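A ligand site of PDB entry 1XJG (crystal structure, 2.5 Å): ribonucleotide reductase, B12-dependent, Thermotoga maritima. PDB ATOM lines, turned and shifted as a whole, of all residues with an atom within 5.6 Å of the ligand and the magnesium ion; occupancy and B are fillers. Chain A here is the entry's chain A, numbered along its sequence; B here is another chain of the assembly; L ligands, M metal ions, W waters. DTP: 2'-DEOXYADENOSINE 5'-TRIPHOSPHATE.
O of Ser 142 lies close to O2A of the ligand, 2.5 Å away. An oxygen (O2A) of the ligand lies within salt-bridge range of the side-chain amino group of Lys 158 of chain B, at 3.7 Å. The guanidinium group of Arg 171 lies within salt-bridge range of an oxygen (O2G) of the ligand. The backbone NH (N) of Ala 178 is in hydrogen-bond range of an oxygen (O1G) of the ligand (3.5 Å). The backbone carbonyl oxygen of Lys 202 of chain B lies within hydrogen-bond range of a nitrogen (N6) of the ligand (2.8 Å). OG1 of Thr 180 lies within hydrogen-bond range of N6 of the ligand (3.3 Å). The side-chain carboxylate (OD1) of Asp 141 sits at hydrogen-bond distance from an oxygen (O3') of the ligand (2.9 Å). The backbone NH (N) of Lys 202 of chain B sits at hydrogen-bond distance from a nitrogen (N1) of the ligand, at 3.2 Å.
O of Lys 158 of chain B is in hydrogen-bond range of OG1 of Thr 180 (2.7 Å). O of Val 200 of chain B sits at hydrogen-bond distance from OG of Ser 185 (2.6 Å). The guanidinium group of Arg 171 is in salt-bridge range of the side-chain carboxylate of Asp 141, 2.7 Å away. NH1 of Arg 171 is in hydrogen-bond range of O of Phe 176 (3.3 Å).
O of Lys 183 lies close to N3 of the ligand (3.4 Å). Residues that only touch the ligand: Ile 143 (3.1 Å), Ala 184 (3.5 Å), Ser 185 (3.5 Å), Gly 179 (3.5 Å), Val 201 of chain B (3.6 Å), Val 177 (3.7 Å), Phe 190 (3.7 Å), Val 200 of chain B (3.8 Å) and Ile 146 (3.8 Å). Within 4 Å of the ligand: Asp 141, Ser 142, Ile 143, Ile 146, Arg 171, Val 177, Ala 178, Gly 179, Thr 180, Lys 183, Ala 184, Ser 185, Phe 190, Lys 158 of chain B, Val 200 of chain B, Val 201 of chain B and Lys 202 of chain B. Along chain A the residues within 4 Å of the ligand span positions 141 to 190.
Residues that only touch the magnesium ion: Ser 142 (3.7 Å). Of the 23 residues printed, 1 comes within 4 Å of the magnesium ion. The nearest printed residue that does not touch the magnesium ion is Asp 141 (4.5 Å).
The magnesium ion is bound by an oxygen (O2B) of the ligand. The magnesium ion has one donor atom within binding distance. Slightly farther from the magnesium ion lies O1A of the ligand (2.7 Å).
Water W1 bridges the backbone carbonyl oxygen (O) of Arg 171 and an oxygen (O3') of the ligand.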
ATOM      1  N   ASP A 141       1.450 -21.672  -9.999  1.00  0.00           N
ATOM      2  CA  ASP A 141       2.559 -20.829 -10.398  1.00  0.00           C
ATOM      3  C   ASP A 141       3.969 -21.366 -10.083  1.00  0.00           C
ATOM      4  O   ASP A 141       4.740 -20.652  -9.424  1.00  0.00           O
ATOM      5  CB  ASP A 141       2.396 -19.448  -9.768  1.00  0.00           C
ATOM      6  CG  ASP A 141       3.173 -18.403 -10.499  1.00  0.00           C
ATOM      7  OD1 ASP A 141       3.454 -18.655 -11.681  1.00  0.00           O
ATOM      8  OD2 ASP A 141       3.532 -17.355  -9.915  1.00  0.00           O
ATOM      9  N   SER A 142       4.345 -22.561 -10.547  1.00  0.00           N
ATOM     10  CA  SER A 142       5.522 -23.172  -9.914  1.00  0.00           C
ATOM     11  C   SER A 142       6.557 -24.083 -10.611  1.00  0.00           C
ATOM     12  O   SER A 142       7.578 -24.399  -9.992  1.00  0.00           O
ATOM     13  CB  SER A 142       5.115 -23.820  -8.575  1.00  0.00           C
ATOM     14  OG  SER A 142       5.060 -25.213  -8.711  1.00  0.00           O
ATOM     15  N   ILE A 143       6.363 -24.524 -11.853  1.00  0.00           N
ATOM     16  CA  ILE A 143       7.345 -25.492 -12.475  1.00  0.00           C
ATOM     17  C   ILE A 143       7.028 -26.905 -12.048  1.00  0.00           C
ATOM     18  O   ILE A 143       6.603 -27.691 -12.887  1.00  0.00           O
ATOM     19  CB  ILE A 143       8.851 -25.185 -12.200  1.00  0.00           C
ATOM     20  CG1 ILE A 143       9.248 -23.820 -12.741  1.00  0.00           C
ATOM     21  CG2 ILE A 143       9.745 -26.182 -12.914  1.00  0.00           C
ATOM     22  CD1 ILE A 143       9.800 -23.856 -14.131  1.00  0.00           C
ATOM     23  N   GLU A 144       7.195 -27.242 -10.765  1.00  0.00           N
ATOM     24  CA  GLU A 144       6.691 -28.531 -10.279  1.00  0.00           C
ATOM     25  C   GLU A 144       5.257 -28.744 -10.751  1.00  0.00           C
ATOM     26  O   GLU A 144       4.916 -29.742 -11.357  1.00  0.00           O
ATOM     27  CB  GLU A 144       6.684 -28.567  -8.759  1.00  0.00           C
ATOM     28  CG  GLU A 144       7.301 -29.786  -8.073  1.00  0.00           C
ATOM     29  CD  GLU A 144       6.691 -31.128  -8.472  1.00  0.00           C
ATOM     30  OE1 GLU A 144       5.438 -31.263  -8.470  1.00  0.00           O
ATOM     31  OE2 GLU A 144       7.501 -32.065  -8.760  1.00  0.00           O
ATOM     32  N   ILE A 146       3.452 -26.674 -13.083  1.00  0.00           N
ATOM     33  CA  ILE A 146       3.402 -26.519 -14.547  1.00  0.00           C
ATOM     34  C   ILE A 146       3.680 -27.856 -15.230  1.00  0.00           C
ATOM     35  O   ILE A 146       2.848 -28.385 -15.983  1.00  0.00           O
ATOM     36  CB  ILE A 146       4.430 -25.500 -15.045  1.00  0.00           C
ATOM     37  CG1 ILE A 146       4.208 -24.113 -14.402  1.00  0.00           C
ATOM     38  CG2 ILE A 146       4.463 -25.463 -16.609  1.00  0.00           C
ATOM     39  CD1 ILE A 146       4.995 -22.940 -15.105  1.00  0.00           C
ATOM     40  N   LEU A 170       0.046 -18.382 -13.760  1.00  0.00           N
ATOM     41  CA  LEU A 170       1.420 -18.165 -14.206  1.00  0.00           C
ATOM     42  C   LEU A 170       1.803 -16.682 -14.212  1.00  0.00           C
ATOM     43  O   LEU A 170       1.177 -15.901 -14.942  1.00  0.00           O
ATOM     44  CB  LEU A 170       1.626 -18.756 -15.610  1.00  0.00           C
ATOM     45  CG  LEU A 170       1.260 -20.252 -15.762  1.00  0.00           C
ATOM     46  CD1 LEU A 170       1.984 -20.866 -16.984  1.00  0.00           C
ATOM     47  CD2 LEU A 170       1.466 -21.084 -14.441  1.00  0.00           C
ATOM     48  N   ARG A 171       2.793 -16.278 -13.388  1.00  0.00           N
ATOM     49  CA  ARG A 171       3.190 -14.852 -13.353  1.00  0.00           C
ATOM     50  C   ARG A 171       3.707 -14.358 -14.717  1.00  0.00           C
ATOM     51  O   ARG A 171       4.301 -15.090 -15.489  1.00  0.00           O
ATOM     52  CB  ARG A 171       4.180 -14.556 -12.211  1.00  0.00           C
ATOM     53  CG  ARG A 171       5.640 -15.040 -12.461  1.00  0.00           C
ATOM     54  CD  ARG A 171       6.477 -15.177 -11.172  1.00  0.00           C
ATOM     55  NE  ARG A 171       5.912 -16.123 -10.189  1.00  0.00           N
ATOM     56  CZ  ARG A 171       6.593 -16.551  -9.122  1.00  0.00           C
ATOM     57  NH1 ARG A 171       7.884 -16.183  -8.992  1.00  0.00           N
ATOM     58  NH2 ARG A 171       6.060 -17.404  -8.220  1.00  0.00           N
ATOM     59  N   PHE A 176      10.235 -11.396 -11.741  1.00  0.00           N
ATOM     60  CA  PHE A 176      11.272 -11.911 -10.854  1.00  0.00           C
ATOM     61  C   PHE A 176      10.941 -13.346 -10.377  1.00  0.00           C
ATOM     62  O   PHE A 176       9.814 -13.644  -9.981  1.00  0.00           O
ATOM     63  CB  PHE A 176      11.457 -10.967  -9.646  1.00  0.00           C
ATOM     64  CG  PHE A 176      12.131 -11.623  -8.451  1.00  0.00           C
ATOM     65  CD1 PHE A 176      13.514 -11.480  -8.230  1.00  0.00           C
ATOM     66  CD2 PHE A 176      11.377 -12.428  -7.551  1.00  0.00           C
ATOM     67  CE1 PHE A 176      14.130 -12.122  -7.130  1.00  0.00           C
ATOM     68  CE2 PHE A 176      11.983 -13.084  -6.449  1.00  0.00           C
ATOM     69  CZ  PHE A 176      13.365 -12.934  -6.236  1.00  0.00           C
ATOM     70  N   VAL A 177      11.954 -14.196 -10.383  1.00  0.00           N
ATOM     71  CA  VAL A 177      11.873 -15.537  -9.778  1.00  0.00           C
ATOM     72  C   VAL A 177      13.113 -15.689  -8.943  1.00  0.00           C
ATOM     73  O   VAL A 177      14.223 -15.334  -9.394  1.00  0.00           O
ATOM     74  CB  VAL A 177      12.015 -16.696 -10.853  1.00  0.00           C
ATOM     75  CG1 VAL A 177      11.456 -18.035 -10.313  1.00  0.00           C
ATOM     76  CG2 VAL A 177      11.427 -16.301 -12.234  1.00  0.00           C
ATOM     77  N   ALA A 178      12.953 -16.248  -7.753  1.00  0.00           N
ATOM     78  CA  ALA A 178      14.111 -16.881  -7.112  1.00  0.00           C
ATOM     79  C   ALA A 178      13.642 -17.868  -6.067  1.00  0.00           C
ATOM     80  O   ALA A 178      13.072 -17.441  -5.064  1.00  0.00           O
ATOM     81  CB  ALA A 178      15.143 -15.832  -6.524  1.00  0.00           C
ATOM     82  N   GLY A 179      13.715 -19.174  -6.341  1.00  0.00           N
ATOM     83  CA  GLY A 179      13.694 -19.740  -7.697  1.00  0.00           C
ATOM     84  C   GLY A 179      14.951 -20.230  -8.434  1.00  0.00           C
ATOM     85  O   GLY A 179      15.291 -21.429  -8.383  1.00  0.00           O
ATOM     86  N   THR A 180      15.601 -19.307  -9.133  1.00  0.00           N
ATOM     87  CA  THR A 180      16.449 -19.630 -10.273  1.00  0.00           C
ATOM     88  C   THR A 180      17.257 -18.395 -10.616  1.00  0.00           C
ATOM     89  O   THR A 180      18.441 -18.471 -10.982  1.00  0.00           O
ATOM     90  CB  THR A 180      15.561 -19.953 -11.524  1.00  0.00           C
ATOM     91  OG1 THR A 180      15.347 -21.355 -11.639  1.00  0.00           O
ATOM     92  CG2 THR A 180      16.225 -19.472 -12.815  1.00  0.00           C
ATOM     93  N   GLY A 182      16.309 -16.469 -13.492  1.00  0.00           N
ATOM     94  CA  GLY A 182      16.390 -16.376 -14.961  1.00  0.00           C
ATOM     95  C   GLY A 182      15.318 -15.480 -15.616  1.00  0.00           C
ATOM     96  O   GLY A 182      15.439 -15.154 -16.825  1.00  0.00           O
ATOM     97  N   LYS A 183      14.307 -15.065 -14.837  1.00  0.00           N
ATOM     98  CA  LYS A 183      13.057 -14.391 -15.371  1.00  0.00           C
ATOM     99  C   LYS A 183      11.986 -15.399 -15.828  1.00  0.00           C
ATOM    100  O   LYS A 183      12.293 -16.417 -16.477  1.00  0.00           O
ATOM    101  CB  LYS A 183      13.337 -13.385 -16.506  1.00  0.00           C
ATOM    102  CG  LYS A 183      13.499 -11.943 -16.046  1.00  0.00           C
ATOM    103  CD  LYS A 183      14.544 -11.169 -16.851  1.00  0.00           C
ATOM    104  CE  LYS A 183      14.975  -9.895 -16.103  1.00  0.00           C
ATOM    105  NZ  LYS A 183      14.786 -10.039 -14.604  1.00  0.00           N
ATOM    106  N   ALA A 184      10.730 -15.126 -15.455  1.00  0.00           N
ATOM    107  CA  ALA A 184       9.584 -15.979 -15.819  1.00  0.00           C
ATOM    108  C   ALA A 184       9.292 -15.876 -17.312  1.00  0.00           C
ATOM    109  O   ALA A 184       9.277 -14.777 -17.896  1.00  0.00           O
ATOM    110  CB  ALA A 184       8.337 -15.645 -14.999  1.00  0.00           C
ATOM    111  N   SER A 185       9.081 -17.021 -17.937  1.00  0.00           N
ATOM    112  CA  SER A 185       8.826 -17.059 -19.363  1.00  0.00           C
ATOM    113  C   SER A 185       7.462 -16.487 -19.731  1.00  0.00           C
ATOM    114  O   SER A 185       7.308 -16.017 -20.852  1.00  0.00           O
ATOM    115  CB  SER A 185       8.941 -18.484 -19.862  1.00  0.00           C
ATOM    116  OG  SER A 185      10.268 -18.914 -19.788  1.00  0.00           O
ATOM    117  N   PHE A 190       4.726 -21.050 -21.711  1.00  0.00           N
ATOM    118  CA  PHE A 190       4.584 -22.370 -21.108  1.00  0.00           C
ATOM    119  C   PHE A 190       3.501 -23.165 -21.776  1.00  0.00           C
ATOM    120  O   PHE A 190       3.503 -24.374 -21.702  1.00  0.00           O
ATOM    121  CB  PHE A 190       4.300 -22.268 -19.634  1.00  0.00           C
ATOM    122  CG  PHE A 190       5.490 -21.840 -18.821  1.00  0.00           C
ATOM    123  CD1 PHE A 190       6.655 -22.611 -18.805  1.00  0.00           C
ATOM    124  CD2 PHE A 190       5.445 -20.685 -18.017  1.00  0.00           C
ATOM    125  CE1 PHE A 190       7.761 -22.227 -18.042  1.00  0.00           C
ATOM    126  CE2 PHE A 190       6.551 -20.301 -17.254  1.00  0.00           C
ATOM    127  CZ  PHE A 190       7.714 -21.058 -17.266  1.00  0.00           C
ATOM    128  N   LEU B 128      18.064 -23.957  -3.901  1.00  0.00           N
ATOM    129  CA  LEU B 128      18.889 -23.594  -5.086  1.00  0.00           C
ATOM    130  C   LEU B 128      20.378 -23.910  -4.870  1.00  0.00           C
ATOM    131  O   LEU B 128      21.223 -23.549  -5.716  1.00  0.00           O
ATOM    132  CB  LEU B 128      18.747 -22.116  -5.473  1.00  0.00           C
ATOM    133  CG  LEU B 128      17.408 -21.391  -5.289  1.00  0.00           C
ATOM    134  CD1 LEU B 128      17.505 -19.965  -5.937  1.00  0.00           C
ATOM    135  CD2 LEU B 128      16.131 -22.224  -5.777  1.00  0.00           C
ATOM    136  N   LYS B 158      16.245 -25.964 -13.972  1.00  0.00           N
ATOM    137  CA  LYS B 158      15.874 -24.735 -13.217  1.00  0.00           C
ATOM    138  C   LYS B 158      16.955 -24.381 -12.168  1.00  0.00           C
ATOM    139  O   LYS B 158      17.288 -23.232 -11.979  1.00  0.00           O
ATOM    140  CB  LYS B 158      14.462 -24.826 -12.612  1.00  0.00           C
ATOM    141  CG  LYS B 158      14.285 -24.234 -11.224  1.00  0.00           C
ATOM    142  CD  LYS B 158      13.027 -23.366 -11.018  1.00  0.00           C
ATOM    143  CE  LYS B 158      12.747 -23.179  -9.488  1.00  0.00           C
ATOM    144  NZ  LYS B 158      12.459 -24.488  -8.716  1.00  0.00           N
ATOM    145  N   VAL B 200      11.901 -23.264 -22.631  1.00  0.00           N
ATOM    146  CA  VAL B 200      11.097 -22.387 -21.819  1.00  0.00           C
ATOM    147  C   VAL B 200      11.603 -22.254 -20.379  1.00  0.00           C
ATOM    148  O   VAL B 200      11.382 -21.213 -19.774  1.00  0.00           O
ATOM    149  CB  VAL B 200       9.611 -22.815 -21.890  1.00  0.00           C
ATOM    150  CG1 VAL B 200       8.930 -22.674 -20.580  1.00  0.00           C
ATOM    151  CG2 VAL B 200       8.902 -22.054 -23.003  1.00  0.00           C
ATOM    152  N   VAL B 201      12.246 -23.281 -19.829  1.00  0.00           N
ATOM    153  CA  VAL B 201      12.940 -23.145 -18.534  1.00  0.00           C
ATOM    154  C   VAL B 201      14.364 -22.597 -18.706  1.00  0.00           C
ATOM    155  O   VAL B 201      15.216 -23.341 -19.173  1.00  0.00           O
ATOM    156  CB  VAL B 201      13.045 -24.492 -17.753  1.00  0.00           C
ATOM    157  CG1 VAL B 201      13.486 -24.232 -16.350  1.00  0.00           C
ATOM    158  CG2 VAL B 201      11.732 -25.236 -17.719  1.00  0.00           C
ATOM    159  N   LYS B 202      14.639 -21.330 -18.362  1.00  0.00           N
ATOM    160  CA  LYS B 202      16.058 -20.867 -18.251  1.00  0.00           C
ATOM    161  C   LYS B 202      16.889 -21.521 -17.112  1.00  0.00           C
ATOM    162  O   LYS B 202      16.418 -21.589 -15.964  1.00  0.00           O
ATOM    163  CB  LYS B 202      16.195 -19.346 -18.192  1.00  0.00           C
ATOM    164  CG  LYS B 202      16.448 -18.728 -19.575  1.00  0.00           C
ATOM    165  CD  LYS B 202      15.142 -18.316 -20.212  1.00  0.00           C
ATOM    166  CE  LYS B 202      15.101 -18.740 -21.665  1.00  0.00           C
ATOM    167  NZ  LYS B 202      13.690 -18.733 -22.187  1.00  0.00           N
ATOM    168  N   GLN B 203      18.138 -21.943 -17.464  1.00  0.00           N
ATOM    169  CA  GLN B 203      19.088 -22.685 -16.585  1.00  0.00           C
ATOM    170  C   GLN B 203      19.994 -21.788 -15.738  1.00  0.00           C
ATOM    171  O   GLN B 203      19.886 -20.558 -15.766  1.00  0.00           O
ATOM    172  CB  GLN B 203      19.939 -23.647 -17.430  1.00  0.00           C
ATOM    173  CG  GLN B 203      20.940 -24.565 -16.676  1.00  0.00           C
ATOM    174  CD  GLN B 203      21.819 -25.370 -17.651  1.00  0.00           C
ATOM    175  OE1 GLN B 203      22.128 -24.908 -18.755  1.00  0.00           O
ATOM    176  NE2 GLN B 203      22.211 -26.576 -17.243  1.00  0.00           N
HETATM  177  PG  DTP L   1       9.098 -18.126  -6.416  1.00  0.00           P
HETATM  178  O1G DTP L   1       9.646 -16.886  -6.970  1.00  0.00           O
HETATM  179  O2G DTP L   1       7.818 -18.648  -6.888  1.00  0.00           O
HETATM  180  O3G DTP L   1       8.992 -18.015  -4.852  1.00  0.00           O
HETATM  181  PB  DTP L   1       9.750 -20.719  -6.781  1.00  0.00           P
HETATM  182  O1B DTP L   1      10.787 -21.544  -6.180  1.00  0.00           O
HETATM  183  O2B DTP L   1       8.342 -20.886  -6.382  1.00  0.00           O
HETATM  184  O3B DTP L   1      10.189 -19.229  -6.601  1.00  0.00           O
HETATM  185  PA  DTP L   1       8.824 -21.552  -9.231  1.00  0.00           P
HETATM  186  O1A DTP L   1       7.620 -21.655  -8.430  1.00  0.00           O
HETATM  187  O2A DTP L   1       9.423 -22.758  -9.785  1.00  0.00           O
HETATM  188  O3A DTP L   1       9.905 -20.794  -8.357  1.00  0.00           O
HETATM  189  O5' DTP L   1       8.606 -20.565 -10.436  1.00  0.00           O
HETATM  190  C5' DTP L   1       7.485 -19.723 -10.398  1.00  0.00           C
HETATM  191  C4' DTP L   1       7.170 -19.077 -11.724  1.00  0.00           C
HETATM  192  O4' DTP L   1       8.293 -18.621 -12.473  1.00  0.00           O
HETATM  193  C3' DTP L   1       6.399 -20.008 -12.633  1.00  0.00           C
HETATM  194  O3' DTP L   1       5.618 -19.235 -13.541  1.00  0.00           O
HETATM  195  C2' DTP L   1       7.526 -20.620 -13.380  1.00  0.00           C
HETATM  196  C1' DTP L   1       8.414 -19.448 -13.623  1.00  0.00           C
HETATM  197  N9  DTP L   1       9.758 -19.977 -13.593  1.00  0.00           N
HETATM  198  C8  DTP L   1      10.306 -20.654 -12.593  1.00  0.00           C
HETATM  199  N7  DTP L   1      11.546 -20.970 -12.923  1.00  0.00           N
HETATM  200  C5  DTP L   1      11.776 -20.501 -14.127  1.00  0.00           C
HETATM  201  C6  DTP L   1      12.868 -20.534 -14.968  1.00  0.00           C
HETATM  202  N6  DTP L   1      13.973 -21.137 -14.577  1.00  0.00           N
HETATM  203  N1  DTP L   1      12.787 -19.949 -16.151  1.00  0.00           N
HETATM  204  C2  DTP L   1      11.673 -19.345 -16.526  1.00  0.00           C
HETATM  205  N3  DTP L   1      10.605 -19.298 -15.759  1.00  0.00           N
HETATM  206  C4  DTP L   1      10.637 -19.869 -14.557  1.00  0.00           C
HETATM  207 MG    MG M   1       7.042 -22.213  -5.827  1.00  0.00          MG
HETATM  208  O   HOH W   1       5.631 -17.446 -16.353  1.00  0.00           O
